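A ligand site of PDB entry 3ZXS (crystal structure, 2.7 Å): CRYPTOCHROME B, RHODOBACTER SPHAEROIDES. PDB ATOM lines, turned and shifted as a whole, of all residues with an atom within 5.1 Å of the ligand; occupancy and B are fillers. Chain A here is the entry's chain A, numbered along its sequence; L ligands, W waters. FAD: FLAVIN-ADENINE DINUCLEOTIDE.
A ring nitrogen (NE2) of His 275 lies close to a ring nitrogen (ND1) of His 375. The side-chain amide nitrogen of Asn 283 is in hydrogen-bond range of the backbone carbonyl oxygen of Asp 407 (2.9 Å). OD1 of Asn 283 is in hydrogen-bond range of NH2 of Arg 321. The side-chain amide nitrogen (ND2) of Asn 416 lies close to the side-chain sulfur (SD) of Met 420. The backbone carbonyl oxygen (O) of Arg 379 lies within hydrogen-bond range of the side-chain hydroxyl (OH) of Tyr 401, 2.7 Å away. The guanidinium group of Arg 379 lies within hydrogen-bond range of the backbone carbonyl oxygen of Ala 374 (2.8 Å). The backbone carbonyl oxygen (O) of Gln 316 lies within hydrogen-bond range of the backbone NH (N) of Arg 321. OG1 of Thr 417 is in hydrogen-bond range of O of Glu 413, at 2.9 Å.
Water W2 lies within hydrogen-bond range of N5 of the ligand (2.7 Å) and O of Tyr 401 (2.8 Å). Water W3 lies within hydrogen-bond range of an oxygen (O1A) of the ligand (2.7 Å), the backbone NH (N) of His 376 (3.0 Å), a ring nitrogen (ND1) of His 275 (3.3 Å) and the side-chain hydroxyl (OH) of Tyr 373 (3.4 Å). Water W1 lies within hydrogen-bond range of O2 of the ligand (2.8 Å) and NE of Arg 321 (3.3 Å). Water W4 lies within hydrogen-bond range of OE1 of Gln 316 (2.5 Å) and N7A of the ligand (2.8 Å).
The side-chain hydroxyl (OH) of Tyr 373 is in hydrogen-bond range of an oxygen (O1P) of the ligand (2.6 Å). O1A of the ligand sits at hydrogen-bond distance from ND1 of His 275 (2.7 Å). An oxygen (O2A) of the ligand lies within hydrogen-bond range of the backbone NH of Ala 276, at 2.7 Å. The side-chain amide nitrogen of Asn 283 lies within hydrogen-bond range of an oxygen (O2) of the ligand (2.8 Å). The backbone NH of Leu 277 is in hydrogen-bond range of an oxygen (O1P) of the ligand (2.9 Å). An oxygen (O2P) of the ligand is in hydrogen-bond range of the backbone NH (N) of Leu 278. A nitrogen (N3) of the ligand sits at hydrogen-bond distance from the backbone carbonyl oxygen (O) of Asp 407 (3.0 Å). OD1 of Asp 407 is in hydrogen-bond range of N3 of the ligand (3.4 Å). O4' of the ligand sits at hydrogen-bond distance from N of His 376 (3.5 Å). ND1 of His 376 lies within hydrogen-bond range of O2' of the ligand (3.0 Å). The side-chain amide oxygen of Asn 416 lies close to a nitrogen (N1A) of the ligand (3.1 Å). The backbone NH of Ser 279 is in hydrogen-bond range of an oxygen (O2P) of the ligand (3.2 Å). NH1 of Arg 379 sits close to N5 of the ligand (3.4 Å).
Phe 259 touches the ligand (CE1 to O2A, 3.5 Å). Met 282 touches the ligand (CE to O2B, 3.4 Å). CE1 of Phe 313 touches C5B of the ligand (3.6 Å). CB of Gln 316 touches O4B of the ligand (3.3 Å). Ile 317 touches the ligand. Trp 320 touches the ligand. Arg 321 touches the ligand (CB to N3A, 3.5 Å). Ala 374 touches the ligand. His 375 touches the ligand. N of Leu 380 touches C8M of the ligand, at 3.8 Å. Tyr 401 touches the ligand (CE1 to C7M, 3.3 Å). Ala 408 touches the ligand. Val 412 touches the ligand. Glu 413 touches the ligand. OG1 of Thr 417 touches C6 of the ligand (3.6 Å). Of the 30 residues printed, 26 come within 4 Å of the ligand.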
ATOM      1  N   PHE A 259      25.839   1.700 -14.584  1.00  0.00           N
ATOM      2  CA  PHE A 259      25.812   0.364 -13.979  1.00  0.00           C
ATOM      3  C   PHE A 259      25.917  -0.741 -15.009  1.00  0.00           C
ATOM      4  O   PHE A 259      26.614  -1.728 -14.791  1.00  0.00           O
ATOM      5  CB  PHE A 259      24.562   0.186 -13.109  1.00  0.00           C
ATOM      6  CG  PHE A 259      24.484  -1.155 -12.446  1.00  0.00           C
ATOM      7  CD1 PHE A 259      25.072  -1.357 -11.215  1.00  0.00           C
ATOM      8  CD2 PHE A 259      23.865  -2.210 -13.079  1.00  0.00           C
ATOM      9  CE1 PHE A 259      25.023  -2.603 -10.596  1.00  0.00           C
ATOM     10  CE2 PHE A 259      23.817  -3.479 -12.479  1.00  0.00           C
ATOM     11  CZ  PHE A 259      24.385  -3.669 -11.227  1.00  0.00           C
ATOM     12  N   HIS A 275      29.228  -0.164  -8.877  1.00  0.00           N
ATOM     13  CA  HIS A 275      28.280  -1.003  -8.152  1.00  0.00           C
ATOM     14  C   HIS A 275      27.676  -0.237  -7.022  1.00  0.00           C
ATOM     15  O   HIS A 275      28.199   0.772  -6.605  1.00  0.00           O
ATOM     16  CB  HIS A 275      29.006  -2.228  -7.626  1.00  0.00           C
ATOM     17  CG  HIS A 275      29.541  -3.084  -8.720  1.00  0.00           C
ATOM     18  ND1 HIS A 275      28.780  -4.046  -9.344  1.00  0.00           N
ATOM     19  CD2 HIS A 275      30.753  -3.101  -9.335  1.00  0.00           C
ATOM     20  CE1 HIS A 275      29.498  -4.629 -10.274  1.00  0.00           C
ATOM     21  NE2 HIS A 275      30.707  -4.075 -10.296  1.00  0.00           N
ATOM     22  N   ALA A 276      26.573  -0.716  -6.505  1.00  0.00           N
ATOM     23  CA  ALA A 276      25.784   0.080  -5.560  1.00  0.00           C
ATOM     24  C   ALA A 276      26.243  -0.033  -4.116  1.00  0.00           C
ATOM     25  O   ALA A 276      25.928   0.835  -3.296  1.00  0.00           O
ATOM     26  CB  ALA A 276      24.327  -0.315  -5.661  1.00  0.00           C
ATOM     27  N   LEU A 277      26.958  -1.107  -3.779  1.00  0.00           N
ATOM     28  CA  LEU A 277      27.352  -1.342  -2.398  1.00  0.00           C
ATOM     29  C   LEU A 277      26.150  -1.244  -1.398  1.00  0.00           C
ATOM     30  O   LEU A 277      26.243  -0.626  -0.337  1.00  0.00           O
ATOM     31  CB  LEU A 277      28.478  -0.366  -2.004  1.00  0.00           C
ATOM     32  CG  LEU A 277      29.855  -0.846  -2.460  1.00  0.00           C
ATOM     33  CD1 LEU A 277      29.884  -0.863  -3.966  1.00  0.00           C
ATOM     34  CD2 LEU A 277      30.981   0.062  -1.879  1.00  0.00           C
ATOM     35  N   LEU A 278      25.034  -1.868  -1.757  1.00  0.00           N
ATOM     36  CA  LEU A 278      23.774  -1.870  -0.958  1.00  0.00           C
ATOM     37  C   LEU A 278      23.402  -3.221  -0.383  1.00  0.00           C
ATOM     38  O   LEU A 278      22.555  -3.286   0.475  1.00  0.00           O
ATOM     39  CB  LEU A 278      22.572  -1.448  -1.806  1.00  0.00           C
ATOM     40  CG  LEU A 278      22.717  -0.061  -2.430  1.00  0.00           C
ATOM     41  CD1 LEU A 278      21.533   0.168  -3.368  1.00  0.00           C
ATOM     42  CD2 LEU A 278      22.823   1.046  -1.357  1.00  0.00           C
ATOM     43  N   SER A 279      24.034  -4.282  -0.860  1.00  0.00           N
ATOM     44  CA  SER A 279      23.673  -5.615  -0.435  1.00  0.00           C
ATOM     45  C   SER A 279      23.550  -5.767   1.089  1.00  0.00           C
ATOM     46  O   SER A 279      22.611  -6.413   1.557  1.00  0.00           O
ATOM     47  CB  SER A 279      24.658  -6.643  -0.990  1.00  0.00           C
ATOM     48  OG  SER A 279      26.007  -6.269  -0.742  1.00  0.00           O
ATOM     49  N   MET A 282      20.341  -3.944   2.369  1.00  0.00           N
ATOM     50  CA  MET A 282      19.139  -4.695   2.039  1.00  0.00           C
ATOM     51  C   MET A 282      19.036  -5.958   2.877  1.00  0.00           C
ATOM     52  O   MET A 282      17.988  -6.303   3.399  1.00  0.00           O
ATOM     53  CB  MET A 282      19.145  -5.061   0.568  1.00  0.00           C
ATOM     54  CG  MET A 282      18.122  -4.314  -0.218  1.00  0.00           C
ATOM     55  SD  MET A 282      18.103  -4.605  -2.030  1.00  0.00           S
ATOM     56  CE  MET A 282      19.761  -3.983  -2.466  1.00  0.00           C
ATOM     57  N   ASN A 283      20.138  -6.664   3.016  1.00  0.00           N
ATOM     58  CA  ASN A 283      20.102  -7.934   3.667  1.00  0.00           C
ATOM     59  C   ASN A 283      19.783  -7.799   5.149  1.00  0.00           C
ATOM     60  O   ASN A 283      19.133  -8.679   5.691  1.00  0.00           O
ATOM     61  CB  ASN A 283      21.407  -8.690   3.407  1.00  0.00           C
ATOM     62  CG  ASN A 283      21.540  -9.177   1.956  1.00  0.00           C
ATOM     63  OD1 ASN A 283      20.619  -9.033   1.172  1.00  0.00           O
ATOM     64  ND2 ASN A 283      22.703  -9.757   1.601  1.00  0.00           N
ATOM     65  N   PHE A 313      20.311  -3.441 -13.510  1.00  0.00           N
ATOM     66  CA  PHE A 313      20.235  -3.268 -12.092  1.00  0.00           C
ATOM     67  C   PHE A 313      19.029  -4.024 -11.533  1.00  0.00           C
ATOM     68  O   PHE A 313      19.174  -4.877 -10.639  1.00  0.00           O
ATOM     69  CB  PHE A 313      20.177  -1.785 -11.733  1.00  0.00           C
ATOM     70  CG  PHE A 313      20.177  -1.524 -10.265  1.00  0.00           C
ATOM     71  CD1 PHE A 313      21.281  -1.828  -9.503  1.00  0.00           C
ATOM     72  CD2 PHE A 313      19.093  -0.966  -9.635  1.00  0.00           C
ATOM     73  CE1 PHE A 313      21.298  -1.567  -8.150  1.00  0.00           C
ATOM     74  CE2 PHE A 313      19.110  -0.706  -8.283  1.00  0.00           C
ATOM     75  CZ  PHE A 313      20.202  -1.012  -7.539  1.00  0.00           C
ATOM     76  N   GLN A 316      19.185  -7.891 -11.218  1.00  0.00           N
ATOM     77  CA  GLN A 316      19.957  -8.428 -10.131  1.00  0.00           C
ATOM     78  C   GLN A 316      19.100  -8.549  -8.850  1.00  0.00           C
ATOM     79  O   GLN A 316      19.344  -9.455  -8.047  1.00  0.00           O
ATOM     80  CB  GLN A 316      21.220  -7.592  -9.870  1.00  0.00           C
ATOM     81  CG  GLN A 316      22.168  -7.357 -11.077  1.00  0.00           C
ATOM     82  CD  GLN A 316      22.267  -8.526 -12.037  1.00  0.00           C
ATOM     83  OE1 GLN A 316      22.636  -9.624 -11.644  1.00  0.00           O
ATOM     84  NE2 GLN A 316      21.904  -8.287 -13.316  1.00  0.00           N
ATOM     85  N   ILE A 317      18.110  -7.683  -8.664  1.00  0.00           N
ATOM     86  CA  ILE A 317      17.356  -7.668  -7.392  1.00  0.00           C
ATOM     87  C   ILE A 317      16.025  -8.404  -7.512  1.00  0.00           C
ATOM     88  O   ILE A 317      15.643  -9.201  -6.654  1.00  0.00           O
ATOM     89  CB  ILE A 317      17.065  -6.210  -6.914  1.00  0.00           C
ATOM     90  CG1 ILE A 317      18.360  -5.510  -6.520  1.00  0.00           C
ATOM     91  CG2 ILE A 317      16.098  -6.189  -5.749  1.00  0.00           C
ATOM     92  CD1 ILE A 317      18.241  -3.986  -6.524  1.00  0.00           C
ATOM     93  N   TRP A 320      17.639 -12.268  -9.703  1.00  0.00           N
ATOM     94  CA  TRP A 320      18.562 -13.122  -8.965  1.00  0.00           C
ATOM     95  C   TRP A 320      18.395 -13.178  -7.449  1.00  0.00           C
ATOM     96  O   TRP A 320      18.321 -14.264  -6.858  1.00  0.00           O
ATOM     97  CB  TRP A 320      19.977 -12.681  -9.274  1.00  0.00           C
ATOM     98  CG  TRP A 320      20.487 -13.188 -10.564  1.00  0.00           C
ATOM     99  CD1 TRP A 320      20.919 -12.450 -11.600  1.00  0.00           C
ATOM    100  CD2 TRP A 320      20.660 -14.556 -10.932  1.00  0.00           C
ATOM    101  NE1 TRP A 320      21.380 -13.272 -12.604  1.00  0.00           N
ATOM    102  CE2 TRP A 320      21.234 -14.574 -12.215  1.00  0.00           C
ATOM    103  CE3 TRP A 320      20.399 -15.770 -10.303  1.00  0.00           C
ATOM    104  CZ2 TRP A 320      21.520 -15.746 -12.895  1.00  0.00           C
ATOM    105  CZ3 TRP A 320      20.696 -16.950 -10.978  1.00  0.00           C
ATOM    106  CH2 TRP A 320      21.253 -16.930 -12.265  1.00  0.00           C
ATOM    107  N   ARG A 321      18.337 -12.009  -6.809  1.00  0.00           N
ATOM    108  CA  ARG A 321      18.162 -11.976  -5.372  1.00  0.00           C
ATOM    109  C   ARG A 321      16.933 -12.789  -4.957  1.00  0.00           C
ATOM    110  O   ARG A 321      17.049 -13.658  -4.069  1.00  0.00           O
ATOM    111  CB  ARG A 321      18.097 -10.542  -4.840  1.00  0.00           C
ATOM    112  CG  ARG A 321      18.256 -10.481  -3.290  1.00  0.00           C
ATOM    113  CD  ARG A 321      18.311  -9.063  -2.736  1.00  0.00           C
ATOM    114  NE  ARG A 321      18.432  -9.052  -1.289  1.00  0.00           N
ATOM    115  CZ  ARG A 321      17.420  -8.905  -0.442  1.00  0.00           C
ATOM    116  NH1 ARG A 321      16.173  -8.724  -0.893  1.00  0.00           N
ATOM    117  NH2 ARG A 321      17.635  -8.900   0.864  1.00  0.00           N
ATOM    118  N   VAL A 324      17.389 -16.662  -5.878  1.00  0.00           N
ATOM    119  CA  VAL A 324      18.291 -17.236  -4.899  1.00  0.00           C
ATOM    120  C   VAL A 324      17.575 -17.502  -3.588  1.00  0.00           C
ATOM    121  O   VAL A 324      17.781 -18.521  -3.008  1.00  0.00           O
ATOM    122  CB  VAL A 324      19.513 -16.330  -4.656  1.00  0.00           C
ATOM    123  CG1 VAL A 324      20.182 -16.664  -3.328  1.00  0.00           C
ATOM    124  CG2 VAL A 324      20.535 -16.455  -5.807  1.00  0.00           C
ATOM    125  N   TYR A 373      34.498  -6.580   0.913  1.00  0.00           N
ATOM    126  CA  TYR A 373      33.690  -6.457  -0.253  1.00  0.00           C
ATOM    127  C   TYR A 373      34.437  -6.790  -1.550  1.00  0.00           C
ATOM    128  O   TYR A 373      35.507  -6.285  -1.818  1.00  0.00           O
ATOM    129  CB  TYR A 373      33.143  -5.033  -0.332  1.00  0.00           C
ATOM    130  CG  TYR A 373      32.388  -4.779  -1.593  1.00  0.00           C
ATOM    131  CD1 TYR A 373      31.048  -5.076  -1.676  1.00  0.00           C
ATOM    132  CD2 TYR A 373      33.019  -4.291  -2.728  1.00  0.00           C
ATOM    133  CE1 TYR A 373      30.350  -4.873  -2.840  1.00  0.00           C
ATOM    134  CE2 TYR A 373      32.306  -4.101  -3.903  1.00  0.00           C
ATOM    135  CZ  TYR A 373      30.971  -4.404  -3.968  1.00  0.00           C
ATOM    136  OH  TYR A 373      30.225  -4.190  -5.135  1.00  0.00           O
ATOM    137  N   ALA A 374      33.823  -7.630  -2.378  1.00  0.00           N
ATOM    138  CA  ALA A 374      34.277  -7.876  -3.741  1.00  0.00           C
ATOM    139  C   ALA A 374      33.037  -7.738  -4.592  1.00  0.00           C
ATOM    140  O   ALA A 374      31.994  -8.213  -4.190  1.00  0.00           O
ATOM    141  CB  ALA A 374      34.888  -9.276  -3.894  1.00  0.00           C
ATOM    142  N   HIS A 375      33.085  -7.090  -5.756  1.00  0.00           N
ATOM    143  CA  HIS A 375      31.876  -7.065  -6.577  1.00  0.00           C
ATOM    144  C   HIS A 375      31.647  -8.413  -7.296  1.00  0.00           C
ATOM    145  O   HIS A 375      32.536  -9.292  -7.356  1.00  0.00           O
ATOM    146  CB  HIS A 375      31.814  -5.867  -7.539  1.00  0.00           C
ATOM    147  CG  HIS A 375      32.999  -5.702  -8.415  1.00  0.00           C
ATOM    148  ND1 HIS A 375      33.136  -6.352  -9.624  1.00  0.00           N
ATOM    149  CD2 HIS A 375      34.123  -4.951  -8.280  1.00  0.00           C
ATOM    150  CE1 HIS A 375      34.289  -6.032 -10.166  1.00  0.00           C
ATOM    151  NE2 HIS A 375      34.911  -5.170  -9.377  1.00  0.00           N
ATOM    152  N   HIS A 376      30.454  -8.564  -7.839  1.00  0.00           N
ATOM    153  CA  HIS A 376      29.976  -9.824  -8.320  1.00  0.00           C
ATOM    154  C   HIS A 376      30.940 -10.615  -9.241  1.00  0.00           C
ATOM    155  O   HIS A 376      31.177 -11.823  -9.028  1.00  0.00           O
ATOM    156  CB  HIS A 376      28.633  -9.601  -9.001  1.00  0.00           C
ATOM    157  CG  HIS A 376      27.992 -10.854  -9.473  1.00  0.00           C
ATOM    158  ND1 HIS A 376      27.429 -11.766  -8.606  1.00  0.00           N
ATOM    159  CD2 HIS A 376      27.883 -11.394 -10.712  1.00  0.00           C
ATOM    160  CE1 HIS A 376      26.976 -12.800  -9.306  1.00  0.00           C
ATOM    161  NE2 HIS A 376      27.261 -12.605 -10.583  1.00  0.00           N
ATOM    162  N   ARG A 379      33.628 -12.307  -7.407  1.00  0.00           N
ATOM    163  CA  ARG A 379      33.171 -13.451  -6.638  1.00  0.00           C
ATOM    164  C   ARG A 379      32.942 -14.681  -7.560  1.00  0.00           C
ATOM    165  O   ARG A 379      33.276 -15.823  -7.202  1.00  0.00           O
ATOM    166  CB  ARG A 379      31.882 -13.115  -5.884  1.00  0.00           C
ATOM    167  CG  ARG A 379      31.982 -11.929  -4.948  1.00  0.00           C
ATOM    168  CD  ARG A 379      30.817 -11.885  -3.933  1.00  0.00           C
ATOM    169  NE  ARG A 379      30.641 -10.549  -3.333  1.00  0.00           N
ATOM    170  CZ  ARG A 379      29.870 -10.251  -2.281  1.00  0.00           C
ATOM    171  NH1 ARG A 379      29.184 -11.174  -1.654  1.00  0.00           N
ATOM    172  NH2 ARG A 379      29.780  -9.014  -1.839  1.00  0.00           N
ATOM    173  N   LEU A 380      32.426 -14.423  -8.752  1.00  0.00           N
ATOM    174  CA  LEU A 380      32.072 -15.470  -9.696  1.00  0.00           C
ATOM    175  C   LEU A 380      33.275 -15.898 -10.518  1.00  0.00           C
ATOM    176  O   LEU A 380      33.699 -17.031 -10.449  1.00  0.00           O
ATOM    177  CB  LEU A 380      30.946 -14.961 -10.615  1.00  0.00           C
ATOM    178  CG  LEU A 380      30.283 -15.924 -11.599  1.00  0.00           C
ATOM    179  CD1 LEU A 380      29.679 -17.090 -10.902  1.00  0.00           C
ATOM    180  CD2 LEU A 380      29.259 -15.194 -12.489  1.00  0.00           C
ATOM    181  N   TYR A 401      32.981 -17.873   1.658  1.00  0.00           N
ATOM    182  CA  TYR A 401      32.097 -16.812   1.194  1.00  0.00           C
ATOM    183  C   TYR A 401      31.125 -16.382   2.296  1.00  0.00           C
ATOM    184  O   TYR A 401      30.712 -15.242   2.336  1.00  0.00           O
ATOM    185  CB  TYR A 401      31.282 -17.217  -0.022  1.00  0.00           C
ATOM    186  CG  TYR A 401      32.032 -17.090  -1.312  1.00  0.00           C
ATOM    187  CD1 TYR A 401      32.041 -15.920  -2.009  1.00  0.00           C
ATOM    188  CD2 TYR A 401      32.756 -18.155  -1.809  1.00  0.00           C
ATOM    189  CE1 TYR A 401      32.769 -15.775  -3.188  1.00  0.00           C
ATOM    190  CE2 TYR A 401      33.488 -18.027  -2.962  1.00  0.00           C
ATOM    191  CZ  TYR A 401      33.480 -16.857  -3.664  1.00  0.00           C
ATOM    192  OH  TYR A 401      34.179 -16.790  -4.848  1.00  0.00           O
ATOM    193  N   ASP A 407      28.055  -8.717   3.296  1.00  0.00           N
ATOM    194  CA  ASP A 407      26.657  -8.974   2.979  1.00  0.00           C
ATOM    195  C   ASP A 407      26.265 -10.454   3.091  1.00  0.00           C
ATOM    196  O   ASP A 407      25.166 -10.836   2.674  1.00  0.00           O
ATOM    197  CB  ASP A 407      26.357  -8.444   1.567  1.00  0.00           C
ATOM    198  CG  ASP A 407      27.350  -9.006   0.503  1.00  0.00           C
ATOM    199  OD1 ASP A 407      28.062 -10.002   0.834  1.00  0.00           O
ATOM    200  OD2 ASP A 407      27.437  -8.438  -0.634  1.00  0.00           O
ATOM    201  N   ALA A 408      27.131 -11.277   3.683  1.00  0.00           N
ATOM    202  CA  ALA A 408      26.931 -12.750   3.671  1.00  0.00           C
ATOM    203  C   ALA A 408      26.063 -13.263   4.818  1.00  0.00           C
ATOM    204  O   ALA A 408      26.340 -13.019   6.007  1.00  0.00           O
ATOM    205  CB  ALA A 408      28.268 -13.477   3.631  1.00  0.00           C
ATOM    206  N   LEU A 409      24.964 -13.897   4.428  1.00  0.00           N
ATOM    207  CA  LEU A 409      24.130 -14.736   5.315  1.00  0.00           C
ATOM    208  C   LEU A 409      23.735 -15.967   4.533  1.00  0.00           C
ATOM    209  O   LEU A 409      23.718 -15.964   3.310  1.00  0.00           O
ATOM    210  CB  LEU A 409      22.898 -13.987   5.747  1.00  0.00           C
ATOM    211  CG  LEU A 409      23.116 -12.568   6.328  1.00  0.00           C
ATOM    212  CD1 LEU A 409      21.816 -11.770   6.248  1.00  0.00           C
ATOM    213  CD2 LEU A 409      23.632 -12.649   7.764  1.00  0.00           C
ATOM    214  N   VAL A 412      21.401 -16.052   1.142  1.00  0.00           N
ATOM    215  CA  VAL A 412      21.835 -15.432  -0.108  1.00  0.00           C
ATOM    216  C   VAL A 412      23.181 -15.976  -0.564  1.00  0.00           C
ATOM    217  O   VAL A 412      23.427 -16.134  -1.757  1.00  0.00           O
ATOM    218  CB  VAL A 412      21.900 -13.883   0.025  1.00  0.00           C
ATOM    219  CG1 VAL A 412      22.729 -13.461   1.220  1.00  0.00           C
ATOM    220  CG2 VAL A 412      22.409 -13.255  -1.246  1.00  0.00           C
ATOM    221  N   GLU A 413      24.071 -16.262   0.371  1.00  0.00           N
ATOM    222  CA  GLU A 413      25.370 -16.818   0.014  1.00  0.00           C
ATOM    223  C   GLU A 413      25.298 -18.263  -0.511  1.00  0.00           C
ATOM    224  O   GLU A 413      26.022 -18.614  -1.433  1.00  0.00           O
ATOM    225  CB  GLU A 413      26.306 -16.738   1.207  1.00  0.00           C
ATOM    226  CG  GLU A 413      27.573 -17.496   1.003  1.00  0.00           C
ATOM    227  CD  GLU A 413      27.436 -18.933   1.433  1.00  0.00           C
ATOM    228  OE1 GLU A 413      26.692 -19.196   2.392  1.00  0.00           O
ATOM    229  OE2 GLU A 413      28.077 -19.812   0.814  1.00  0.00           O
ATOM    230  N   ASN A 416      24.337 -18.918  -4.298  1.00  0.00           N
ATOM    231  CA  ASN A 416      25.339 -18.294  -5.164  1.00  0.00           C
ATOM    232  C   ASN A 416      26.617 -19.104  -5.159  1.00  0.00           C
ATOM    233  O   ASN A 416      27.244 -19.235  -6.198  1.00  0.00           O
ATOM    234  CB  ASN A 416      25.598 -16.862  -4.768  1.00  0.00           C
ATOM    235  CG  ASN A 416      24.549 -15.898  -5.289  1.00  0.00           C
ATOM    236  OD1 ASN A 416      23.883 -15.189  -4.521  1.00  0.00           O
ATOM    237  ND2 ASN A 416      24.391 -15.858  -6.598  1.00  0.00           N
ATOM    238  N   THR A 417      26.966 -19.695  -4.023  1.00  0.00           N
ATOM    239  CA  THR A 417      28.256 -20.369  -3.845  1.00  0.00           C
ATOM    240  C   THR A 417      28.183 -21.838  -4.246  1.00  0.00           C
ATOM    241  O   THR A 417      28.935 -22.307  -5.061  1.00  0.00           O
ATOM    242  CB  THR A 417      28.767 -20.197  -2.401  1.00  0.00           C
ATOM    243  OG1 THR A 417      28.860 -18.784  -2.091  1.00  0.00           O
ATOM    244  CG2 THR A 417      30.147 -20.826  -2.215  1.00  0.00           C
ATOM    245  N   MET A 420      25.477 -21.460  -8.302  1.00  0.00           N
ATOM    246  CA  MET A 420      26.036 -20.628  -9.347  1.00  0.00           C
ATOM    247  C   MET A 420      27.520 -20.825  -9.524  1.00  0.00           C
ATOM    248  O   MET A 420      27.952 -21.055 -10.623  1.00  0.00           O
ATOM    249  CB  MET A 420      25.777 -19.123  -9.094  1.00  0.00           C
ATOM    250  CG  MET A 420      25.912 -18.245 -10.342  1.00  0.00           C
ATOM    251  SD  MET A 420      25.590 -16.475 -10.027  1.00  0.00           S
ATOM    252  CE  MET A 420      23.823 -16.556  -9.698  1.00  0.00           C
ATOM    253  N   SER A 421      28.296 -20.765  -8.452  1.00  0.00           N
ATOM    254  CA  SER A 421      29.737 -20.733  -8.607  1.00  0.00           C
ATOM    255  C   SER A 421      30.374 -22.113  -8.641  1.00  0.00           C
ATOM    256  O   SER A 421      31.142 -22.434  -9.568  1.00  0.00           O
ATOM    257  CB  SER A 421      30.368 -19.880  -7.517  1.00  0.00           C
ATOM    258  OG  SER A 421      31.786 -19.935  -7.627  1.00  0.00           O
HETATM  259  PA  FAD L   1      25.546  -4.592  -7.238  1.00  0.00           P
HETATM  260  O1A FAD L   1      26.493  -5.035  -8.271  1.00  0.00           O
HETATM  261  O2A FAD L   1      25.432  -3.107  -7.135  1.00  0.00           O
HETATM  262  O5B FAD L   1      24.137  -5.291  -7.552  1.00  0.00           O
HETATM  263  C5B FAD L   1      22.983  -4.616  -7.081  1.00  0.00           C
HETATM  264  C4B FAD L   1      22.203  -5.465  -6.104  1.00  0.00           C
HETATM  265  O4B FAD L   1      21.710  -6.624  -6.767  1.00  0.00           O
HETATM  266  C3B FAD L   1      22.998  -5.955  -4.911  1.00  0.00           C
HETATM  267  O3B FAD L   1      23.085  -5.046  -3.841  1.00  0.00           O
HETATM  268  C2B FAD L   1      22.241  -7.201  -4.543  1.00  0.00           C
HETATM  269  O2B FAD L   1      21.176  -6.865  -3.694  1.00  0.00           O
HETATM  270  C1B FAD L   1      21.673  -7.695  -5.831  1.00  0.00           C
HETATM  271  N9A FAD L   1      22.391  -8.835  -6.416  1.00  0.00           N
HETATM  272  C8A FAD L   1      23.210  -8.863  -7.527  1.00  0.00           C
HETATM  273  N7A FAD L   1      23.579 -10.138  -7.772  1.00  0.00           N
HETATM  274  C5A FAD L   1      22.955 -10.910  -6.852  1.00  0.00           C
HETATM  275  C6A FAD L   1      22.982 -12.277  -6.603  1.00  0.00           C
HETATM  276  N6A FAD L   1      23.440 -13.104  -7.532  1.00  0.00           N
HETATM  277  N1A FAD L   1      22.303 -12.774  -5.522  1.00  0.00           N
HETATM  278  C2A FAD L   1      21.561 -11.949  -4.725  1.00  0.00           C
HETATM  279  N3A FAD L   1      21.549 -10.583  -4.945  1.00  0.00           N
HETATM  280  C4A FAD L   1      22.236 -10.095  -6.000  1.00  0.00           C
HETATM  281  N1  FAD L   1      25.107 -11.383  -2.467  1.00  0.00           N
HETATM  282  C2  FAD L   1      24.725 -11.070  -1.181  1.00  0.00           C
HETATM  283  O2  FAD L   1      23.895 -10.193  -0.910  1.00  0.00           O
HETATM  284  N3  FAD L   1      25.259 -11.750  -0.154  1.00  0.00           N
HETATM  285  C4  FAD L   1      26.157 -12.734  -0.360  1.00  0.00           C
HETATM  286  O4  FAD L   1      26.601 -13.296   0.645  1.00  0.00           O
HETATM  287  C4X FAD L   1      26.549 -13.054  -1.641  1.00  0.00           C
HETATM  288  N5  FAD L   1      27.482 -14.065  -1.845  1.00  0.00           N
HETATM  289  C5X FAD L   1      27.865 -14.363  -3.148  1.00  0.00           C
HETATM  290  C6  FAD L   1      28.792 -15.381  -3.353  1.00  0.00           C
HETATM  291  C7  FAD L   1      29.185 -15.739  -4.634  1.00  0.00           C
HETATM  292  C7M FAD L   1      30.175 -16.840  -4.864  1.00  0.00           C
HETATM  293  C8  FAD L   1      28.678 -15.026  -5.703  1.00  0.00           C
HETATM  294  C8M FAD L   1      29.117 -15.383  -7.097  1.00  0.00           C
HETATM  295  C9  FAD L   1      27.744 -14.016  -5.499  1.00  0.00           C
HETATM  296  C9A FAD L   1      27.331 -13.679  -4.228  1.00  0.00           C
HETATM  297  N10 FAD L   1      26.424 -12.653  -3.995  1.00  0.00           N
HETATM  298  C10 FAD L   1      26.027 -12.368  -2.702  1.00  0.00           C
HETATM  299  C1' FAD L   1      25.793 -11.879  -5.125  1.00  0.00           C
HETATM  300  C2' FAD L   1      26.498 -10.592  -5.519  1.00  0.00           C
HETATM  301  O2' FAD L   1      27.832 -10.869  -5.796  1.00  0.00           O
HETATM  302  C3' FAD L   1      26.385  -9.524  -4.433  1.00  0.00           C
HETATM  303  O3' FAD L   1      25.021  -9.430  -4.097  1.00  0.00           O
HETATM  304  C4' FAD L   1      26.950  -8.179  -4.863  1.00  0.00           C
HETATM  305  O4' FAD L   1      28.338  -8.341  -5.064  1.00  0.00           O
HETATM  306  C5' FAD L   1      26.738  -7.124  -3.795  1.00  0.00           C
HETATM  307  O5' FAD L   1      27.446  -5.956  -4.129  1.00  0.00           O
HETATM  308  P   FAD L   1      26.663  -4.622  -4.580  1.00  0.00           P
HETATM  309  O1P FAD L   1      27.714  -3.642  -4.973  1.00  0.00           O
HETATM  310  O2P FAD L   1      25.701  -4.090  -3.568  1.00  0.00           O
HETATM  311  O3P FAD L   1      25.851  -5.227  -5.807  1.00  0.00           O
HETATM  312  O   HOH W   1      21.568  -9.575  -2.275  1.00  0.00           O
HETATM  313  O   HOH W   2      29.239 -14.151   0.222  1.00  0.00           O
HETATM  314  O   HOH W   3      28.516  -6.410  -7.091  1.00  0.00           O
HETATM  315  O   HOH W   4      24.703 -10.159 -10.303  1.00  0.00           O
